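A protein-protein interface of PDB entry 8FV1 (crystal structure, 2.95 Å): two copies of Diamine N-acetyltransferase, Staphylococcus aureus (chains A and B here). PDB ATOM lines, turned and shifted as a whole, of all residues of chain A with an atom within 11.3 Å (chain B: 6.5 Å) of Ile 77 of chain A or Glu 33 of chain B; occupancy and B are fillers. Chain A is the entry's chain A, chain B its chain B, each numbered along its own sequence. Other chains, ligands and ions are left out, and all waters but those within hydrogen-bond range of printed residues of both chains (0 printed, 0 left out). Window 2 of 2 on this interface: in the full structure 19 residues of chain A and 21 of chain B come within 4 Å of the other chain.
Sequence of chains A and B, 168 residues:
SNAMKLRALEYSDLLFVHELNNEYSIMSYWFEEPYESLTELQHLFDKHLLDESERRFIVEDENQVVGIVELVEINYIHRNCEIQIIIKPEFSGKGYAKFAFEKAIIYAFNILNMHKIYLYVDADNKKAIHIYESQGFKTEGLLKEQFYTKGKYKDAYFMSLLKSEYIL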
ATOM      1  N   GLU A  52      13.719   7.271  -3.447  1.00  0.00           N
ATOM      2  CA  GLU A  52      14.819   6.317  -3.450  1.00  0.00           C
ATOM      3  C   GLU A  52      16.178   6.979  -3.633  1.00  0.00           C
ATOM      4  O   GLU A  52      17.201   6.296  -3.511  1.00  0.00           O
ATOM      5  CB  GLU A  52      14.605   5.273  -4.548  1.00  0.00           C
ATOM      6  CG  GLU A  52      13.293   4.513  -4.428  1.00  0.00           C
ATOM      7  CD  GLU A  52      13.177   3.747  -3.123  1.00  0.00           C
ATOM      8  OE1 GLU A  52      14.212   3.533  -2.460  1.00  0.00           O
ATOM      9  OE2 GLU A  52      12.046   3.361  -2.758  1.00  0.00           O
ATOM     10  N   SER A  53      16.217   8.279  -3.923  1.00  0.00           N
ATOM     11  CA  SER A  53      17.476   9.007  -4.000  1.00  0.00           C
ATOM     12  C   SER A  53      18.036   9.356  -2.628  1.00  0.00           C
ATOM     13  O   SER A  53      19.074  10.023  -2.554  1.00  0.00           O
ATOM     14  CB  SER A  53      17.294  10.287  -4.818  1.00  0.00           C
ATOM     15  OG  SER A  53      16.385  11.171  -4.185  1.00  0.00           O
ATOM     16  N   GLU A  73      21.198  12.135  -2.770  1.00  0.00           N
ATOM     17  CA  GLU A  73      21.506  12.311  -4.189  1.00  0.00           C
ATOM     18  C   GLU A  73      22.019  11.010  -4.802  1.00  0.00           C
ATOM     19  O   GLU A  73      22.976  10.996  -5.578  1.00  0.00           O
ATOM     20  CB  GLU A  73      22.511  13.445  -4.390  1.00  0.00           C
ATOM     21  CG  GLU A  73      22.012  14.804  -3.918  1.00  0.00           C
ATOM     22  CD  GLU A  73      20.847  15.319  -4.742  1.00  0.00           C
ATOM     23  OE1 GLU A  73      20.575  14.742  -5.816  1.00  0.00           O
ATOM     24  OE2 GLU A  73      20.201  16.299  -4.314  1.00  0.00           O
ATOM     25  N   ILE A  74      21.369   9.904  -4.446  1.00  0.00           N
ATOM     26  CA  ILE A  74      21.764   8.588  -4.941  1.00  0.00           C
ATOM     27  C   ILE A  74      21.366   8.500  -6.411  1.00  0.00           C
ATOM     28  O   ILE A  74      20.178   8.428  -6.738  1.00  0.00           O
ATOM     29  CB  ILE A  74      21.119   7.465  -4.122  1.00  0.00           C
ATOM     30  CG1 ILE A  74      21.461   7.622  -2.637  1.00  0.00           C
ATOM     31  CG2 ILE A  74      21.584   6.106  -4.630  1.00  0.00           C
ATOM     32  CD1 ILE A  74      20.636   6.737  -1.722  1.00  0.00           C
ATOM     33  N   ASN A  75      22.356   8.504  -7.300  1.00  0.00           N
ATOM     34  CA  ASN A  75      22.128   8.409  -8.736  1.00  0.00           C
ATOM     35  C   ASN A  75      22.368   6.969  -9.171  1.00  0.00           C
ATOM     36  O   ASN A  75      23.474   6.444  -9.009  1.00  0.00           O
ATOM     37  CB  ASN A  75      23.043   9.369  -9.494  1.00  0.00           C
ATOM     38  CG  ASN A  75      22.544   9.669 -10.893  1.00  0.00           C
ATOM     39  OD1 ASN A  75      22.284   8.758 -11.678  1.00  0.00           O
ATOM     40  ND2 ASN A  75      22.396  10.951 -11.208  1.00  0.00           N
ATOM     41  N   TYR A  76      21.333   6.333  -9.714  1.00  0.00           N
ATOM     42  CA  TYR A  76      21.390   4.928 -10.096  1.00  0.00           C
ATOM     43  C   TYR A  76      21.835   4.719 -11.541  1.00  0.00           C
ATOM     44  O   TYR A  76      21.756   3.594 -12.040  1.00  0.00           O
ATOM     45  CB  TYR A  76      20.025   4.272  -9.860  1.00  0.00           C
ATOM     46  CG  TYR A  76      19.651   4.179  -8.398  1.00  0.00           C
ATOM     47  CD1 TYR A  76      20.163   3.167  -7.597  1.00  0.00           C
ATOM     48  CD2 TYR A  76      18.798   5.106  -7.817  1.00  0.00           C
ATOM     49  CE1 TYR A  76      19.835   3.080  -6.259  1.00  0.00           C
ATOM     50  CE2 TYR A  76      18.463   5.026  -6.478  1.00  0.00           C
ATOM     51  CZ  TYR A  76      18.984   4.011  -5.704  1.00  0.00           C
ATOM     52  OH  TYR A  76      18.650   3.930  -4.372  1.00  0.00           O
ATOM     53  N   ILE A  77      22.287   5.780 -12.221  1.00  0.00           N
ATOM     54  CA  ILE A  77      22.914   5.651 -13.535  1.00  0.00           C
ATOM     55  C   ILE A  77      24.431   5.830 -13.427  1.00  0.00           C
ATOM     56  O   ILE A  77      25.198   4.968 -13.883  1.00  0.00           O
ATOM     57  CB  ILE A  77      22.312   6.661 -14.535  1.00  0.00           C
ATOM     58  CG1 ILE A  77      20.832   6.345 -14.795  1.00  0.00           C
ATOM     59  CG2 ILE A  77      23.109   6.661 -15.832  1.00  0.00           C
ATOM     60  CD1 ILE A  77      20.097   7.435 -15.555  1.00  0.00           C
ATOM     61  N   HIS A  78      24.885   6.946 -12.850  1.00  0.00           N
ATOM     62  CA  HIS A  78      26.311   7.171 -12.622  1.00  0.00           C
ATOM     63  C   HIS A  78      26.814   6.474 -11.365  1.00  0.00           C
ATOM     64  O   HIS A  78      28.031   6.372 -11.172  1.00  0.00           O
ATOM     65  CB  HIS A  78      26.588   8.673 -12.534  1.00  0.00           C
ATOM     66  CG  HIS A  78      25.873   9.471 -13.580  1.00  0.00           C
ATOM     67  ND1 HIS A  78      26.003   9.213 -14.928  1.00  0.00           N
ATOM     68  CD2 HIS A  78      25.005  10.505 -13.478  1.00  0.00           C
ATOM     69  CE1 HIS A  78      25.253  10.058 -15.611  1.00  0.00           C
ATOM     70  NE2 HIS A  78      24.636  10.854 -14.755  1.00  0.00           N
ATOM     71  N   ARG A  79      25.903   5.978 -10.528  1.00  0.00           N
ATOM     72  CA  ARG A  79      26.248   5.254  -9.311  1.00  0.00           C
ATOM     73  C   ARG A  79      27.168   6.092  -8.422  1.00  0.00           C
ATOM     74  O   ARG A  79      28.292   5.706  -8.098  1.00  0.00           O
ATOM     75  CB  ARG A  79      26.878   3.898  -9.645  1.00  0.00           C
ATOM     76  CG  ARG A  79      26.073   3.091 -10.650  1.00  0.00           C
ATOM     77  CD  ARG A  79      26.157   1.595 -10.384  1.00  0.00           C
ATOM     78  NE  ARG A  79      27.460   1.027 -10.707  1.00  0.00           N
ATOM     79  CZ  ARG A  79      27.742  -0.269 -10.660  1.00  0.00           C
ATOM     80  NH1 ARG A  79      26.837  -1.159 -10.289  1.00  0.00           N
ATOM     81  NH2 ARG A  79      28.960  -0.681 -11.000  1.00  0.00           N
ATOM     82  N   ASN A  80      26.667   7.264  -8.042  1.00  0.00           N
ATOM     83  CA  ASN A  80      27.349   8.116  -7.078  1.00  0.00           C
ATOM     84  C   ASN A  80      26.327   8.657  -6.087  1.00  0.00           C
ATOM     85  O   ASN A  80      25.201   8.992  -6.463  1.00  0.00           O
ATOM     86  CB  ASN A  80      28.106   9.266  -7.768  1.00  0.00           C
ATOM     87  CG  ASN A  80      27.198  10.202  -8.546  1.00  0.00           C
ATOM     88  OD1 ASN A  80      26.071  10.484  -8.143  1.00  0.00           O
ATOM     89  ND2 ASN A  80      27.697  10.700  -9.671  1.00  0.00           N
ATOM     90  N   CYS A  81      26.726   8.715  -4.814  1.00  0.00           N
ATOM     91  CA  CYS A  81      25.873   9.211  -3.742  1.00  0.00           C
ATOM     92  C   CYS A  81      26.676  10.134  -2.838  1.00  0.00           C
ATOM     93  O   CYS A  81      27.843   9.863  -2.541  1.00  0.00           O
ATOM     94  CB  CYS A  81      25.289   8.065  -2.901  1.00  0.00           C
ATOM     95  SG  CYS A  81      26.519   7.134  -1.958  1.00  0.00           S
ATOM     96  N   LEU A 112      23.934  -0.771  -1.669  1.00  0.00           N
ATOM     97  CA  LEU A 112      23.432   0.073  -2.746  1.00  0.00           C
ATOM     98  C   LEU A 112      24.216  -0.101  -4.042  1.00  0.00           C
ATOM     99  O   LEU A 112      23.841   0.495  -5.056  1.00  0.00           O
ATOM    100  CB  LEU A 112      23.457   1.540  -2.317  1.00  0.00           C
ATOM    101  CG  LEU A 112      22.579   1.887  -1.111  1.00  0.00           C
ATOM    102  CD1 LEU A 112      22.719   3.359  -0.748  1.00  0.00           C
ATOM    103  CD2 LEU A 112      21.120   1.539  -1.378  1.00  0.00           C
ATOM    104  N   ASN A 113      25.285  -0.900  -4.030  1.00  0.00           N
ATOM    105  CA  ASN A 113      26.060  -1.192  -5.235  1.00  0.00           C
ATOM    106  C   ASN A 113      26.505   0.094  -5.927  1.00  0.00           C
ATOM    107  O   ASN A 113      26.490   0.204  -7.155  1.00  0.00           O
ATOM    108  CB  ASN A 113      25.263  -2.080  -6.193  1.00  0.00           C
ATOM    109  CG  ASN A 113      26.125  -2.681  -7.288  1.00  0.00           C
ATOM    110  OD1 ASN A 113      27.353  -2.609  -7.235  1.00  0.00           O
ATOM    111  ND2 ASN A 113      25.484  -3.284  -8.282  1.00  0.00           N
ATOM    112  N   MET A 114      26.908   1.076  -5.129  1.00  0.00           N
ATOM    113  CA  MET A 114      27.370   2.344  -5.674  1.00  0.00           C
ATOM    114  C   MET A 114      28.825   2.234  -6.114  1.00  0.00           C
ATOM    115  O   MET A 114      29.609   1.452  -5.568  1.00  0.00           O
ATOM    116  CB  MET A 114      27.219   3.460  -4.642  1.00  0.00           C
ATOM    117  CG  MET A 114      25.789   3.668  -4.167  1.00  0.00           C
ATOM    118  SD  MET A 114      24.638   4.031  -5.508  1.00  0.00           S
ATOM    119  CE  MET A 114      25.110   5.705  -5.927  1.00  0.00           C
ATOM    120  N   HIS A 115      29.180   3.035  -7.118  1.00  0.00           N
ATOM    121  CA  HIS A 115      30.519   3.024  -7.689  1.00  0.00           C
ATOM    122  C   HIS A 115      31.420   4.112  -7.125  1.00  0.00           C
ATOM    123  O   HIS A 115      32.644   4.016  -7.267  1.00  0.00           O
ATOM    124  CB  HIS A 115      30.433   3.177  -9.213  1.00  0.00           C
ATOM    125  CG  HIS A 115      31.763   3.196  -9.897  1.00  0.00           C
ATOM    126  ND1 HIS A 115      32.153   4.219 -10.735  1.00  0.00           N
ATOM    127  CD2 HIS A 115      32.794   2.319  -9.870  1.00  0.00           C
ATOM    128  CE1 HIS A 115      33.365   3.969 -11.195  1.00  0.00           C
ATOM    129  NE2 HIS A 115      33.778   2.824 -10.685  1.00  0.00           N
ATOM    130  N   LYS A 116      30.852   5.129  -6.482  1.00  0.00           N
ATOM    131  CA  LYS A 116      31.631   6.240  -5.957  1.00  0.00           C
ATOM    132  C   LYS A 116      30.793   6.974  -4.923  1.00  0.00           C
ATOM    133  O   LYS A 116      29.579   7.112  -5.087  1.00  0.00           O
ATOM    134  CB  LYS A 116      32.056   7.192  -7.082  1.00  0.00           C
ATOM    135  CG  LYS A 116      32.673   8.503  -6.614  1.00  0.00           C
ATOM    136  CD  LYS A 116      33.108   9.349  -7.805  1.00  0.00           C
ATOM    137  CE  LYS A 116      33.765  10.648  -7.367  1.00  0.00           C
ATOM    138  NZ  LYS A 116      34.133  11.501  -8.533  1.00  0.00           N
ATOM    139  N   TYR A 118      30.756  10.683  -2.673  1.00  0.00           N
ATOM    140  CA  TYR A 118      31.330  12.022  -2.669  1.00  0.00           C
ATOM    141  C   TYR A 118      30.739  12.825  -1.518  1.00  0.00           C
ATOM    142  O   TYR A 118      29.776  12.414  -0.868  1.00  0.00           O
ATOM    143  CB  TYR A 118      31.109  12.739  -4.011  1.00  0.00           C
ATOM    144  CG  TYR A 118      29.662  12.955  -4.400  1.00  0.00           C
ATOM    145  CD1 TYR A 118      28.900  11.921  -4.929  1.00  0.00           C
ATOM    146  CD2 TYR A 118      29.066  14.202  -4.263  1.00  0.00           C
ATOM    147  CE1 TYR A 118      27.581  12.117  -5.293  1.00  0.00           C
ATOM    148  CE2 TYR A 118      27.748  14.409  -4.626  1.00  0.00           C
ATOM    149  CZ  TYR A 118      27.010  13.364  -5.140  1.00  0.00           C
ATOM    150  OH  TYR A 118      25.698  13.566  -5.501  1.00  0.00           O
ATOM    151  N   ASN B  21      16.600  16.654 -26.807  1.00  0.00           N
ATOM    152  CA  ASN B  21      16.887  15.858 -25.621  1.00  0.00           C
ATOM    153  C   ASN B  21      16.901  14.359 -25.887  1.00  0.00           C
ATOM    154  O   ASN B  21      17.241  13.592 -24.979  1.00  0.00           O
ATOM    155  CB  ASN B  21      15.864  16.169 -24.522  1.00  0.00           C
ATOM    156  CG  ASN B  21      16.064  17.542 -23.911  1.00  0.00           C
ATOM    157  OD1 ASN B  21      16.898  18.323 -24.369  1.00  0.00           O
ATOM    158  ND2 ASN B  21      15.295  17.845 -22.872  1.00  0.00           N
ATOM    159  N   ASN B  22      16.547  13.924 -27.094  1.00  0.00           N
ATOM    160  CA  ASN B  22      16.584  12.513 -27.456  1.00  0.00           C
ATOM    161  C   ASN B  22      17.735  12.185 -28.403  1.00  0.00           C
ATOM    162  O   ASN B  22      17.772  11.082 -28.959  1.00  0.00           O
ATOM    163  CB  ASN B  22      15.253  12.092 -28.087  1.00  0.00           C
ATOM    164  CG  ASN B  22      14.140  11.963 -27.064  1.00  0.00           C
ATOM    165  OD1 ASN B  22      14.018  10.940 -26.389  1.00  0.00           O
ATOM    166  ND2 ASN B  22      13.318  13.000 -26.948  1.00  0.00           N
ATOM    167  N   GLU B  23      18.670  13.111 -28.598  1.00  0.00           N
ATOM    168  CA  GLU B  23      19.830  12.879 -29.446  1.00  0.00           C
ATOM    169  C   GLU B  23      20.961  12.320 -28.589  1.00  0.00           C
ATOM    170  O   GLU B  23      21.461  13.003 -27.688  1.00  0.00           O
ATOM    171  CB  GLU B  23      20.258  14.172 -30.142  1.00  0.00           C
ATOM    172  CG  GLU B  23      21.451  14.013 -31.073  1.00  0.00           C
ATOM    173  CD  GLU B  23      21.188  13.037 -32.204  1.00  0.00           C
ATOM    174  OE1 GLU B  23      20.044  12.996 -32.701  1.00  0.00           O
ATOM    175  OE2 GLU B  23      22.125  12.307 -32.590  1.00  0.00           O
ATOM    176  N   MET B  27      23.173  14.291 -25.627  1.00  0.00           N
ATOM    177  CA  MET B  27      23.022  13.949 -24.218  1.00  0.00           C
ATOM    178  C   MET B  27      24.276  13.286 -23.660  1.00  0.00           C
ATOM    179  O   MET B  27      24.556  13.405 -22.462  1.00  0.00           O
ATOM    180  CB  MET B  27      21.816  13.030 -24.025  1.00  0.00           C
ATOM    181  CG  MET B  27      20.489  13.618 -24.484  1.00  0.00           C
ATOM    182  SD  MET B  27      20.078  15.196 -23.709  1.00  0.00           S
ATOM    183  CE  MET B  27      20.736  16.348 -24.912  1.00  0.00           C
ATOM    184  N   SER B  28      25.037  12.585 -24.502  1.00  0.00           N
ATOM    185  CA  SER B  28      26.248  11.923 -24.023  1.00  0.00           C
ATOM    186  C   SER B  28      27.220  12.933 -23.425  1.00  0.00           C
ATOM    187  O   SER B  28      27.716  12.750 -22.307  1.00  0.00           O
ATOM    188  CB  SER B  28      26.907  11.149 -25.164  1.00  0.00           C
ATOM    189  OG  SER B  28      28.103  10.524 -24.731  1.00  0.00           O
ATOM    190  N   PHE B  31      26.094  14.299 -20.214  1.00  0.00           N
ATOM    191  CA  PHE B  31      25.967  13.257 -19.200  1.00  0.00           C
ATOM    192  C   PHE B  31      24.518  12.855 -18.951  1.00  0.00           C
ATOM    193  O   PHE B  31      24.227  12.180 -17.957  1.00  0.00           O
ATOM    194  CB  PHE B  31      26.618  13.679 -17.873  1.00  0.00           C
ATOM    195  CG  PHE B  31      28.093  13.949 -17.979  1.00  0.00           C
ATOM    196  CD1 PHE B  31      28.966  12.955 -18.389  1.00  0.00           C
ATOM    197  CD2 PHE B  31      28.609  15.193 -17.656  1.00  0.00           C
ATOM    198  CE1 PHE B  31      30.323  13.198 -18.484  1.00  0.00           C
ATOM    199  CE2 PHE B  31      29.965  15.443 -17.748  1.00  0.00           C
ATOM    200  CZ  PHE B  31      30.823  14.444 -18.162  1.00  0.00           C
ATOM    201  N   GLU B  32      23.601  13.248 -19.832  1.00  0.00           N
ATOM    202  CA  GLU B  32      22.193  12.924 -19.688  1.00  0.00           C
ATOM    203  C   GLU B  32      21.879  11.618 -20.414  1.00  0.00           C
ATOM    204  O   GLU B  32      22.752  10.972 -21.001  1.00  0.00           O
ATOM    205  CB  GLU B  32      21.330  14.066 -20.222  1.00  0.00           C
ATOM    206  CG  GLU B  32      21.462  15.367 -19.446  1.00  0.00           C
ATOM    207  CD  GLU B  32      20.759  15.320 -18.105  1.00  0.00           C
ATOM    208  OE1 GLU B  32      20.221  14.249 -17.751  1.00  0.00           O
ATOM    209  OE2 GLU B  32      20.740  16.355 -17.405  1.00  0.00           O
ATOM    210  N   GLU B  33      20.608  11.223 -20.374  1.00  0.00           N
ATOM    211  CA  GLU B  33      20.132  10.033 -21.062  1.00  0.00           C
ATOM    212  C   GLU B  33      19.307  10.440 -22.272  1.00  0.00           C
ATOM    213  O   GLU B  33      18.468  11.344 -22.160  1.00  0.00           O
ATOM    214  CB  GLU B  33      19.289   9.171 -20.115  1.00  0.00           C
ATOM    215  CG  GLU B  33      18.738   7.911 -20.756  1.00  0.00           C
ATOM    216  CD  GLU B  33      18.016   7.022 -19.764  1.00  0.00           C
ATOM    217  OE1 GLU B  33      17.979   7.371 -18.565  1.00  0.00           O
ATOM    218  OE2 GLU B  33      17.486   5.972 -20.184  1.00  0.00           O
ATOM    219  N   PRO B  34      19.515   9.817 -23.451  1.00  0.00           N
ATOM    220  CA  PRO B  34      18.750  10.177 -24.652  1.00  0.00           C
ATOM    221  C   PRO B  34      17.366   9.530 -24.707  1.00  0.00           C
ATOM    222  O   PRO B  34      16.995   8.889 -25.691  1.00  0.00           O
ATOM    223  CB  PRO B  34      19.655   9.685 -25.788  1.00  0.00           C
ATOM    224  CG  PRO B  34      20.337   8.491 -25.211  1.00  0.00           C
ATOM    225  CD  PRO B  34      20.522   8.773 -23.736  1.00  0.00           C
ATOM    226  N   TYR B  35      16.596   9.698 -23.632  1.00  0.00           N
ATOM    227  CA  TYR B  35      15.245   9.152 -23.545  1.00  0.00           C
ATOM    228  C   TYR B  35      14.389  10.138 -22.764  1.00  0.00           C
ATOM    229  O   TYR B  35      14.622  10.355 -21.570  1.00  0.00           O
ATOM    230  CB  TYR B  35      15.241   7.777 -22.875  1.00  0.00           C
ATOM    231  CG  TYR B  35      13.914   7.053 -22.968  1.00  0.00           C
ATOM    232  CD1 TYR B  35      12.820   7.463 -22.217  1.00  0.00           C
ATOM    233  CD2 TYR B  35      13.758   5.956 -23.805  1.00  0.00           C
ATOM    234  CE1 TYR B  35      11.608   6.805 -22.301  1.00  0.00           C
ATOM    235  CE2 TYR B  35      12.550   5.290 -23.894  1.00  0.00           C
ATOM    236  CZ  TYR B  35      11.478   5.718 -23.140  1.00  0.00           C
ATOM    237  OH  TYR B  35      10.274   5.060 -23.226  1.00  0.00           O
ATOM    238  N   GLU B  36      13.402  10.729 -23.433  1.00  0.00           N
ATOM    239  CA  GLU B  36      12.462  11.627 -22.773  1.00  0.00           C
ATOM    240  C   GLU B  36      11.254  11.863 -23.671  1.00  0.00           C
ATOM    241  O   GLU B  36      11.282  12.740 -24.540  1.00  0.00           O
ATOM    242  CB  GLU B  36      13.133  12.955 -22.422  1.00  0.00           C
ATOM    243  CG  GLU B  36      12.273  13.870 -21.560  1.00  0.00           C
ATOM    244  CD  GLU B  36      12.928  15.211 -21.296  1.00  0.00           C
ATOM    245  OE1 GLU B  36      13.616  15.726 -22.202  1.00  0.00           O
ATOM    246  OE2 GLU B  36      12.759  15.749 -20.181  1.00  0.00           O
ATOM    247  N   PHE B 147      30.717  10.318 -13.843  1.00  0.00           N
ATOM    248  CA  PHE B 147      29.574  10.041 -14.704  1.00  0.00           C
ATOM    249  C   PHE B 147      29.792   8.732 -15.446  1.00  0.00           C
ATOM    250  O   PHE B 147      30.886   8.172 -15.451  1.00  0.00           O
ATOM    251  CB  PHE B 147      29.340  11.196 -15.685  1.00  0.00           C
ATOM    252  CG  PHE B 147      29.044  12.503 -15.007  1.00  0.00           C
ATOM    253  CD1 PHE B 147      27.821  12.718 -14.395  1.00  0.00           C
ATOM    254  CD2 PHE B 147      29.992  13.513 -14.972  1.00  0.00           C
ATOM    255  CE1 PHE B 147      27.546  13.915 -13.765  1.00  0.00           C
ATOM    256  CE2 PHE B 147      29.720  14.715 -14.343  1.00  0.00           C
ATOM    257  CZ  PHE B 147      28.496  14.915 -13.739  1.00  0.00           C
ATOM    258  N   TYR B 148      28.726   8.236 -16.069  1.00  0.00           N
ATOM    259  CA  TYR B 148      28.778   6.989 -16.831  1.00  0.00           C
ATOM    260  C   TYR B 148      28.015   7.204 -18.129  1.00  0.00           C
ATOM    261  O   TYR B 148      26.792   7.380 -18.109  1.00  0.00           O
ATOM    262  CB  TYR B 148      28.188   5.823 -16.041  1.00  0.00           C
ATOM    263  CG  TYR B 148      28.262   4.496 -16.765  1.00  0.00           C
ATOM    264  CD1 TYR B 148      27.239   4.085 -17.611  1.00  0.00           C
ATOM    265  CD2 TYR B 148      29.355   3.654 -16.604  1.00  0.00           C
ATOM    266  CE1 TYR B 148      27.304   2.874 -18.277  1.00  0.00           C
ATOM    267  CE2 TYR B 148      29.429   2.441 -17.264  1.00  0.00           C
ATOM    268  CZ  TYR B 148      28.401   2.056 -18.099  1.00  0.00           C
ATOM    269  OH  TYR B 148      28.469   0.850 -18.758  1.00  0.00           O
ATOM    270  N   TYR B 153      32.962   4.968 -17.578  1.00  0.00           N
ATOM    271  CA  TYR B 153      32.945   5.909 -16.463  1.00  0.00           C
ATOM    272  C   TYR B 153      33.831   7.093 -16.825  1.00  0.00           C
ATOM    273  O   TYR B 153      35.060   6.969 -16.879  1.00  0.00           O
ATOM    274  CB  TYR B 153      33.414   5.239 -15.176  1.00  0.00           C
ATOM    275  CG  TYR B 153      32.324   4.483 -14.453  1.00  0.00           C
ATOM    276  CD1 TYR B 153      31.267   5.155 -13.854  1.00  0.00           C
ATOM    277  CD2 TYR B 153      32.354   3.097 -14.362  1.00  0.00           C
ATOM    278  CE1 TYR B 153      30.267   4.470 -13.192  1.00  0.00           C
ATOM    279  CE2 TYR B 153      31.361   2.403 -13.699  1.00  0.00           C
ATOM    280  CZ  TYR B 153      30.321   3.095 -13.115  1.00  0.00           C
ATOM    281  OH  TYR B 153      29.327   2.409 -12.454  1.00  0.00           O
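NE of Arg 79 of chain A lies within hydrogen-bond range of OH of Tyr 153 of chain B, 2.9 Å away. The backbone carbonyl oxygen (O) of Phe 31 of chain B lies close to a ring nitrogen (NE2) of His 78 of chain A, 3.5 Å away. A ring nitrogen (ND1) of His 78 of chain A is in hydrogen-bond range of the backbone NH (N) of Tyr 148 of chain B, at 3.1 Å.
The side-chain amide oxygen (OD1) of Asn 75 of chain A sits at hydrogen-bond distance from the backbone NH (N) of Ile 77 of chain A (3.0 Å). The backbone carbonyl oxygen (O) of Arg 79 of chain A is in hydrogen-bond range of the backbone NH (N) of Lys 116 of chain A, 3.1 Å away. N of His 115 of chain A is in hydrogen-bond range of O of Arg 79 of chain A (3.0 Å). ND2 of Asn 113 of chain A sits close to NH1 of Arg 79 of chain A (3.2 Å). The side-chain amide oxygen (OD1) of Asn 75 of chain A lies within hydrogen-bond range of the backbone NH (N) of His 78 of chain A (3.4 Å).
Among the printed residues, merely in contact across the chains: His 115 of chain A with Tyr 153 of chain B (3.1 Å), His 78 of chain A with Tyr 153 of chain B (3.6 Å), His 78 of chain A with Phe 147 of chain B (3.7 Å), Ile 77 of chain A with Glu 33 of chain B (3.7 Å) and Ile 77 of chain A with Tyr 148 of chain B (3.8 Å).
Tyr 76 of chain A touches none of the printed residues of chain B. Of chain B, only Glu 33 and Tyr 148 come within 4 Å of Ile 77 of chain A. Printed residues of chain B within 4 Å of His 115 of chain A: Tyr 153. No residue of chain A comes within 4 Å of Asn 22 of chain B. Printed residues of chain A within 4 Å of Phe 31 of chain B: His 78. No residue of chain A comes within 4 Å of Glu 32 of chain B. No residue of chain A comes within 4 Å of Pro 34 of chain B. Printed residues of chain A within 4 Å of Phe 147 of chain B: His 78 (3.7 Å). Of chain A, only Ile 77 (3.8 Å) and His 78 (3.1 Å) come within 4 Å of Tyr 148 of chain B. Of the printed residues of chain A, Tyr 153 of chain B touches His 78, Arg 79 and His 115.
Printed residues of chain B that touch a printed residue of chain A: Phe 31, Glu 33, Phe 147, Tyr 148 and Tyr 153. Hydrophobic or aromatic side chains of chain B that line the printed part of chain A: Phe 147, Tyr 148 and Tyr 153. Among the printed residues, 8 pairs touch across the chains. Among the printed residues, no Asp or Glu carboxylate lies within 4 Å of a Lys or Arg side-chain nitrogen of the other chain.
No position is printed for both chains. Of the 8 pairs that touch across the chains among the printed residues, none has its exchanged pair printed and touching as well.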
